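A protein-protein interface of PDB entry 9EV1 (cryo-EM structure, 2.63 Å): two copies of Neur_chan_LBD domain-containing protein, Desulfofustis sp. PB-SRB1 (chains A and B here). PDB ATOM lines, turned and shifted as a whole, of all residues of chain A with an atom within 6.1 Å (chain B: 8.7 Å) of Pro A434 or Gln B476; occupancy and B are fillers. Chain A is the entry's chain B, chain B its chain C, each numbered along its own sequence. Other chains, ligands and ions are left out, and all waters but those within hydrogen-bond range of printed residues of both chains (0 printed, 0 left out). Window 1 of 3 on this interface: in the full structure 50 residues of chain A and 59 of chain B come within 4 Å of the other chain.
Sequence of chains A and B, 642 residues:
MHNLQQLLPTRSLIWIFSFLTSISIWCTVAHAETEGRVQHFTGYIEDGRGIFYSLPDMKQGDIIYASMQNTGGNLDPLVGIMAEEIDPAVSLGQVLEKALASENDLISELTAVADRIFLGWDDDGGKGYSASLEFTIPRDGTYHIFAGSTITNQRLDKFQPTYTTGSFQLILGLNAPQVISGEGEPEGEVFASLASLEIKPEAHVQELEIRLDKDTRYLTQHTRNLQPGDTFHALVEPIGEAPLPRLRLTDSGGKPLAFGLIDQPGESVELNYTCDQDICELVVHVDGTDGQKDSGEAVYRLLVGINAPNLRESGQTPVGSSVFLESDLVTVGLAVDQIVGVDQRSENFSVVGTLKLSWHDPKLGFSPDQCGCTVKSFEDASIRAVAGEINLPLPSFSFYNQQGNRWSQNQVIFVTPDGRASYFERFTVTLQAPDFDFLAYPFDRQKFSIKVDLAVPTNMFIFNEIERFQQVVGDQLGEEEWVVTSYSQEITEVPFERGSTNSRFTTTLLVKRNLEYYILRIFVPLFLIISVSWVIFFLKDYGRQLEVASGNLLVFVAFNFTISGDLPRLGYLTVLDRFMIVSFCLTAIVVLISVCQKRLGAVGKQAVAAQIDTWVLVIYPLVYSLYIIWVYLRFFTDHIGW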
ATOM      1  N   GLU A 347     -24.458   0.292  10.833  1.00  0.00           N
ATOM      2  CA  GLU A 347     -25.365  -0.469   9.971  1.00  0.00           C
ATOM      3  C   GLU A 347     -26.777   0.122   9.973  1.00  0.00           C
ATOM      4  O   GLU A 347     -27.747  -0.506  10.403  1.00  0.00           O
ATOM      5  CB  GLU A 347     -25.382  -1.950  10.370  1.00  0.00           C
ATOM      6  CG  GLU A 347     -24.037  -2.641  10.231  1.00  0.00           C
ATOM      7  CD  GLU A 347     -24.123  -4.137  10.455  1.00  0.00           C
ATOM      8  OE1 GLU A 347     -25.252  -4.666  10.527  1.00  0.00           O
ATOM      9  OE2 GLU A 347     -23.061  -4.785  10.559  1.00  0.00           O
ATOM     10  N   ASN A 401     -37.960  -1.055  11.721  1.00  0.00           N
ATOM     11  CA  ASN A 401     -36.571  -0.838  12.109  1.00  0.00           C
ATOM     12  C   ASN A 401     -36.244   0.641  12.291  1.00  0.00           C
ATOM     13  O   ASN A 401     -35.111   1.063  12.049  1.00  0.00           O
ATOM     14  CB  ASN A 401     -35.629  -1.464  11.083  1.00  0.00           C
ATOM     15  CG  ASN A 401     -35.848  -2.953  10.927  1.00  0.00           C
ATOM     16  OD1 ASN A 401     -35.305  -3.754  11.686  1.00  0.00           O
ATOM     17  ND2 ASN A 401     -36.646  -3.333   9.935  1.00  0.00           N
ATOM     18  N   GLN A 432     -32.535   0.663  10.644  1.00  0.00           N
ATOM     19  CA  GLN A 432     -31.442  -0.256  10.926  1.00  0.00           C
ATOM     20  C   GLN A 432     -31.365  -1.345   9.863  1.00  0.00           C
ATOM     21  O   GLN A 432     -32.381  -1.819   9.349  1.00  0.00           O
ATOM     22  CB  GLN A 432     -31.617  -0.886  12.306  1.00  0.00           C
ATOM     23  CG  GLN A 432     -31.666   0.121  13.442  1.00  0.00           C
ATOM     24  CD  GLN A 432     -31.872  -0.535  14.792  1.00  0.00           C
ATOM     25  OE1 GLN A 432     -31.967  -1.759  14.890  1.00  0.00           O
ATOM     26  NE2 GLN A 432     -31.944   0.275  15.842  1.00  0.00           N
ATOM     27  N   ALA A 433     -30.139  -1.742   9.534  1.00  0.00           N
ATOM     28  CA  ALA A 433     -29.879  -2.745   8.501  1.00  0.00           C
ATOM     29  C   ALA A 433     -28.885  -3.768   9.029  1.00  0.00           C
ATOM     30  O   ALA A 433     -27.690  -3.723   8.715  1.00  0.00           O
ATOM     31  CB  ALA A 433     -29.368  -2.086   7.219  1.00  0.00           C
ATOM     32  N   PRO A 434     -29.350  -4.716   9.848  1.00  0.00           N
ATOM     33  CA  PRO A 434     -28.438  -5.738  10.388  1.00  0.00           C
ATOM     34  C   PRO A 434     -27.930  -6.724   9.347  1.00  0.00           C
ATOM     35  O   PRO A 434     -27.004  -7.488   9.650  1.00  0.00           O
ATOM     36  CB  PRO A 434     -29.293  -6.443  11.446  1.00  0.00           C
ATOM     37  CG  PRO A 434     -30.693  -6.260  10.968  1.00  0.00           C
ATOM     38  CD  PRO A 434     -30.735  -4.907  10.314  1.00  0.00           C
ATOM     39  N   ASP A 435     -28.499  -6.737   8.142  1.00  0.00           N
ATOM     40  CA  ASP A 435     -28.090  -7.680   7.109  1.00  0.00           C
ATOM     41  C   ASP A 435     -26.937  -7.174   6.251  1.00  0.00           C
ATOM     42  O   ASP A 435     -26.545  -7.868   5.308  1.00  0.00           O
ATOM     43  CB  ASP A 435     -29.281  -8.023   6.212  1.00  0.00           C
ATOM     44  CG  ASP A 435     -30.390  -8.731   6.962  1.00  0.00           C
ATOM     45  OD1 ASP A 435     -30.220  -8.987   8.173  1.00  0.00           O
ATOM     46  OD2 ASP A 435     -31.432  -9.031   6.343  1.00  0.00           O
ATOM     47  N   PHE A 436     -26.400  -5.990   6.541  1.00  0.00           N
ATOM     48  CA  PHE A 436     -25.285  -5.461   5.764  1.00  0.00           C
ATOM     49  C   PHE A 436     -24.086  -6.399   5.821  1.00  0.00           C
ATOM     50  O   PHE A 436     -23.762  -6.962   6.871  1.00  0.00           O
ATOM     51  CB  PHE A 436     -24.886  -4.078   6.279  1.00  0.00           C
ATOM     52  CG  PHE A 436     -25.726  -2.958   5.736  1.00  0.00           C
ATOM     53  CD1 PHE A 436     -26.598  -3.173   4.682  1.00  0.00           C
ATOM     54  CD2 PHE A 436     -25.635  -1.687   6.274  1.00  0.00           C
ATOM     55  CE1 PHE A 436     -27.366  -2.141   4.181  1.00  0.00           C
ATOM     56  CE2 PHE A 436     -26.399  -0.652   5.778  1.00  0.00           C
ATOM     57  CZ  PHE A 436     -27.265  -0.879   4.728  1.00  0.00           C
ATOM     58  N   VAL B 336     -30.720 -10.322  22.844  1.00  0.00           N
ATOM     59  CA  VAL B 336     -29.846  -9.325  22.234  1.00  0.00           C
ATOM     60  C   VAL B 336     -29.857  -9.538  20.727  1.00  0.00           C
ATOM     61  O   VAL B 336     -29.610 -10.651  20.249  1.00  0.00           O
ATOM     62  CB  VAL B 336     -28.415  -9.410  22.792  1.00  0.00           C
ATOM     63  CG1 VAL B 336     -27.476  -8.540  21.975  1.00  0.00           C
ATOM     64  CG2 VAL B 336     -28.392  -8.998  24.252  1.00  0.00           C
ATOM     65  N   ASP B 337     -30.142  -8.472  19.981  1.00  0.00           N
ATOM     66  CA  ASP B 337     -30.214  -8.531  18.527  1.00  0.00           C
ATOM     67  C   ASP B 337     -28.938  -8.045  17.849  1.00  0.00           C
ATOM     68  O   ASP B 337     -28.473  -8.667  16.890  1.00  0.00           O
ATOM     69  CB  ASP B 337     -31.412  -7.716  18.027  1.00  0.00           C
ATOM     70  CG  ASP B 337     -32.739  -8.309  18.456  1.00  0.00           C
ATOM     71  OD1 ASP B 337     -32.816  -9.545  18.614  1.00  0.00           O
ATOM     72  OD2 ASP B 337     -33.707  -7.540  18.632  1.00  0.00           O
ATOM     73  N   GLN B 338     -28.356  -6.947  18.328  1.00  0.00           N
ATOM     74  CA  GLN B 338     -27.186  -6.375  17.678  1.00  0.00           C
ATOM     75  C   GLN B 338     -26.474  -5.431  18.637  1.00  0.00           C
ATOM     76  O   GLN B 338     -27.116  -4.624  19.311  1.00  0.00           O
ATOM     77  CB  GLN B 338     -27.579  -5.624  16.399  1.00  0.00           C
ATOM     78  CG  GLN B 338     -26.419  -4.962  15.678  1.00  0.00           C
ATOM     79  CD  GLN B 338     -26.876  -4.062  14.549  1.00  0.00           C
ATOM     80  OE1 GLN B 338     -28.073  -3.878  14.332  1.00  0.00           O
ATOM     81  NE2 GLN B 338     -25.921  -3.493  13.820  1.00  0.00           N
ATOM     82  N   ILE B 339     -25.150  -5.542  18.686  1.00  0.00           N
ATOM     83  CA  ILE B 339     -24.305  -4.568  19.369  1.00  0.00           C
ATOM     84  C   ILE B 339     -23.957  -3.478  18.363  1.00  0.00           C
ATOM     85  O   ILE B 339     -23.286  -3.742  17.359  1.00  0.00           O
ATOM     86  CB  ILE B 339     -23.039  -5.227  19.935  1.00  0.00           C
ATOM     87  CG1 ILE B 339     -23.409  -6.330  20.927  1.00  0.00           C
ATOM     88  CG2 ILE B 339     -22.146  -4.188  20.595  1.00  0.00           C
ATOM     89  CD1 ILE B 339     -22.216  -7.080  21.477  1.00  0.00           C
ATOM     90  N   VAL B 340     -24.414  -2.255  18.626  1.00  0.00           N
ATOM     91  CA  VAL B 340     -24.364  -1.181  17.641  1.00  0.00           C
ATOM     92  C   VAL B 340     -23.267  -0.170  17.922  1.00  0.00           C
ATOM     93  O   VAL B 340     -23.093   0.768  17.130  1.00  0.00           O
ATOM     94  CB  VAL B 340     -25.723  -0.468  17.519  1.00  0.00           C
ATOM     95  CG1 VAL B 340     -26.763  -1.412  16.938  1.00  0.00           C
ATOM     96  CG2 VAL B 340     -26.175   0.052  18.870  1.00  0.00           C
ATOM     97  N   VAL B 352     -29.175  -3.304  20.965  1.00  0.00           N
ATOM     98  CA  VAL B 352     -30.570  -3.378  20.542  1.00  0.00           C
ATOM     99  C   VAL B 352     -31.093  -4.766  20.888  1.00  0.00           C
ATOM    100  O   VAL B 352     -30.432  -5.770  20.597  1.00  0.00           O
ATOM    101  CB  VAL B 352     -30.724  -3.093  19.037  1.00  0.00           C
ATOM    102  CG1 VAL B 352     -32.186  -3.171  18.626  1.00  0.00           C
ATOM    103  CG2 VAL B 352     -30.140  -1.735  18.688  1.00  0.00           C
ATOM    104  N   GLN B 471     -33.406 -16.838  20.906  1.00  0.00           N
ATOM    105  CA  GLN B 471     -31.987 -16.973  21.196  1.00  0.00           C
ATOM    106  C   GLN B 471     -31.483 -15.717  21.893  1.00  0.00           C
ATOM    107  O   GLN B 471     -31.812 -14.597  21.492  1.00  0.00           O
ATOM    108  CB  GLN B 471     -31.201 -17.220  19.909  1.00  0.00           C
ATOM    109  CG  GLN B 471     -31.554 -18.520  19.208  1.00  0.00           C
ATOM    110  CD  GLN B 471     -30.748 -18.737  17.943  1.00  0.00           C
ATOM    111  OE1 GLN B 471     -29.968 -17.877  17.536  1.00  0.00           O
ATOM    112  NE2 GLN B 471     -30.933 -19.892  17.315  1.00  0.00           N
ATOM    113  N   VAL B 473     -28.413 -14.524  22.047  1.00  0.00           N
ATOM    114  CA  VAL B 473     -27.563 -13.825  21.090  1.00  0.00           C
ATOM    115  C   VAL B 473     -27.958 -14.286  19.693  1.00  0.00           C
ATOM    116  O   VAL B 473     -27.877 -15.479  19.375  1.00  0.00           O
ATOM    117  CB  VAL B 473     -26.072 -14.071  21.367  1.00  0.00           C
ATOM    118  CG1 VAL B 473     -25.207 -13.435  20.287  1.00  0.00           C
ATOM    119  CG2 VAL B 473     -25.693 -13.542  22.743  1.00  0.00           C
ATOM    120  N   GLY B 474     -28.396 -13.342  18.863  1.00  0.00           N
ATOM    121  CA  GLY B 474     -28.885 -13.666  17.535  1.00  0.00           C
ATOM    122  C   GLY B 474     -27.793 -13.562  16.483  1.00  0.00           C
ATOM    123  O   GLY B 474     -26.856 -12.777  16.612  1.00  0.00           O
ATOM    124  N   ASP B 475     -27.932 -14.370  15.436  1.00  0.00           N
ATOM    125  CA  ASP B 475     -26.990 -14.372  14.328  1.00  0.00           C
ATOM    126  C   ASP B 475     -27.412 -13.355  13.275  1.00  0.00           C
ATOM    127  O   ASP B 475     -28.603 -13.177  13.006  1.00  0.00           O
ATOM    128  CB  ASP B 475     -26.894 -15.765  13.702  1.00  0.00           C
ATOM    129  CG  ASP B 475     -28.234 -16.278  13.210  1.00  0.00           C
ATOM    130  OD1 ASP B 475     -29.267 -15.929  13.819  1.00  0.00           O
ATOM    131  OD2 ASP B 475     -28.254 -17.032  12.214  1.00  0.00           O
ATOM    132  N   GLN B 476     -26.424 -12.686  12.683  1.00  0.00           N
ATOM    133  CA  GLN B 476     -26.660 -11.696  11.644  1.00  0.00           C
ATOM    134  C   GLN B 476     -25.709 -11.940  10.482  1.00  0.00           C
ATOM    135  O   GLN B 476     -24.613 -12.479  10.658  1.00  0.00           O
ATOM    136  CB  GLN B 476     -26.482 -10.264  12.173  1.00  0.00           C
ATOM    137  CG  GLN B 476     -27.428  -9.888  13.308  1.00  0.00           C
ATOM    138  CD  GLN B 476     -28.874  -9.777  12.860  1.00  0.00           C
ATOM    139  OE1 GLN B 476     -29.166  -9.722  11.665  1.00  0.00           O
ATOM    140  NE2 GLN B 476     -29.789  -9.740  13.822  1.00  0.00           N
ATOM    141  N   LEU B 477     -26.143 -11.540   9.290  1.00  0.00           N
ATOM    142  CA  LEU B 477     -25.322 -11.701   8.100  1.00  0.00           C
ATOM    143  C   LEU B 477     -24.098 -10.793   8.161  1.00  0.00           C
ATOM    144  O   LEU B 477     -24.147  -9.677   8.684  1.00  0.00           O
ATOM    145  CB  LEU B 477     -26.136 -11.397   6.842  1.00  0.00           C
ATOM    146  CG  LEU B 477     -27.339 -12.304   6.579  1.00  0.00           C
ATOM    147  CD1 LEU B 477     -28.062 -11.885   5.308  1.00  0.00           C
ATOM    148  CD2 LEU B 477     -26.907 -13.759   6.498  1.00  0.00           C
ATOM    149  N   GLY B 478     -22.988 -11.287   7.616  1.00  0.00           N
ATOM    150  CA  GLY B 478     -21.747 -10.542   7.614  1.00  0.00           C
ATOM    151  C   GLY B 478     -20.936 -10.749   8.876  1.00  0.00           C
ATOM    152  O   GLY B 478     -21.335 -11.437   9.821  1.00  0.00           O
ATOM    153  N   GLU B 479     -19.761 -10.130   8.886  1.00  0.00           N
ATOM    154  CA  GLU B 479     -18.849 -10.230  10.012  1.00  0.00           C
ATOM    155  C   GLU B 479     -19.120  -9.121  11.023  1.00  0.00           C
ATOM    156  O   GLU B 479     -19.775  -8.119  10.726  1.00  0.00           O
ATOM    157  CB  GLU B 479     -17.397 -10.162   9.540  1.00  0.00           C
ATOM    158  CG  GLU B 479     -17.015 -11.239   8.538  1.00  0.00           C
ATOM    159  CD  GLU B 479     -17.001 -12.628   9.145  1.00  0.00           C
ATOM    160  OE1 GLU B 479     -16.862 -12.741  10.382  1.00  0.00           O
ATOM    161  OE2 GLU B 479     -17.130 -13.611   8.385  1.00  0.00           O
ATOM    162  N   GLU B 480     -18.602  -9.314  12.233  1.00  0.00           N
ATOM    163  CA  GLU B 480     -18.769  -8.359  13.315  1.00  0.00           C
ATOM    164  C   GLU B 480     -17.410  -8.006  13.904  1.00  0.00           C
ATOM    165  O   GLU B 480     -16.465  -8.798  13.863  1.00  0.00           O
ATOM    166  CB  GLU B 480     -19.692  -8.903  14.417  1.00  0.00           C
ATOM    167  CG  GLU B 480     -21.174  -8.898  14.063  1.00  0.00           C
ATOM    168  CD  GLU B 480     -21.551  -9.986  13.075  1.00  0.00           C
ATOM    169  OE1 GLU B 480     -20.769 -10.945  12.916  1.00  0.00           O
ATOM    170  OE2 GLU B 480     -22.632  -9.879  12.458  1.00  0.00           O
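The backbone carbonyl oxygen (O) of Leu B477 sits close to the backbone carbonyl oxygen (O) of Phe A436.
Hydrophobic or aromatic side chains of chain B within 4 Å of the printed part of chain A: Val B352 and Leu B477.
Along chain B the printed residues that touch a printed residue of chain A span positions 338 to 477.
No position is printed for both chains.
Of the printed residues of chain B, Glu A347 touches Gln B338.
No residue of chain B comes within 4 Å of Ala A433.
Pro A434 touches two residues of chain B.
Of the printed residues of chain B, Asp A435 touches Gln B476 (3.7 Å) and Leu B477 (3.9 Å).
Printed residues of chain B within 4 Å of Phe A436: Leu B477.
Ile B339 touches none of the printed residues of chain A.
Of chain A, only Pro A434 (3.3 Å) and Asp A435 (3.7 Å) come within 4 Å of Gln B476.
The nearest residue of chain B that does not touch Pro A434 is Gln B338 (4.05 Å).
The nearest residue of chain A that does not touch Gln B476 is Glu A347 (6.0 Å).
The nearest printed residue of chain A that does not touch Gln B338 is Pro A434 (4.05 Å).
The backbone carbonyl oxygen (O) of Glu A347 lies within hydrogen-bond range of the backbone NH (N) of Ala A433, 2.8 Å away.
O of Asn A401 sits at hydrogen-bond distance from N of Gln A432.
O of Val B352 is in hydrogen-bond range of N of Asp B337 (2.8 Å).
The backbone carbonyl oxygen (O) of Gln B338 is in hydrogen-bond range of the backbone NH (N) of Val B352.
Among the printed residues, merely in contact across the chains: Glu A347 with Gln B338, Gln A432 with Val B352, Pro A434 with Gln B476, Pro A434 with Leu B477, Asp A435 with Gln B476 and Asp A435 with Leu B477.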
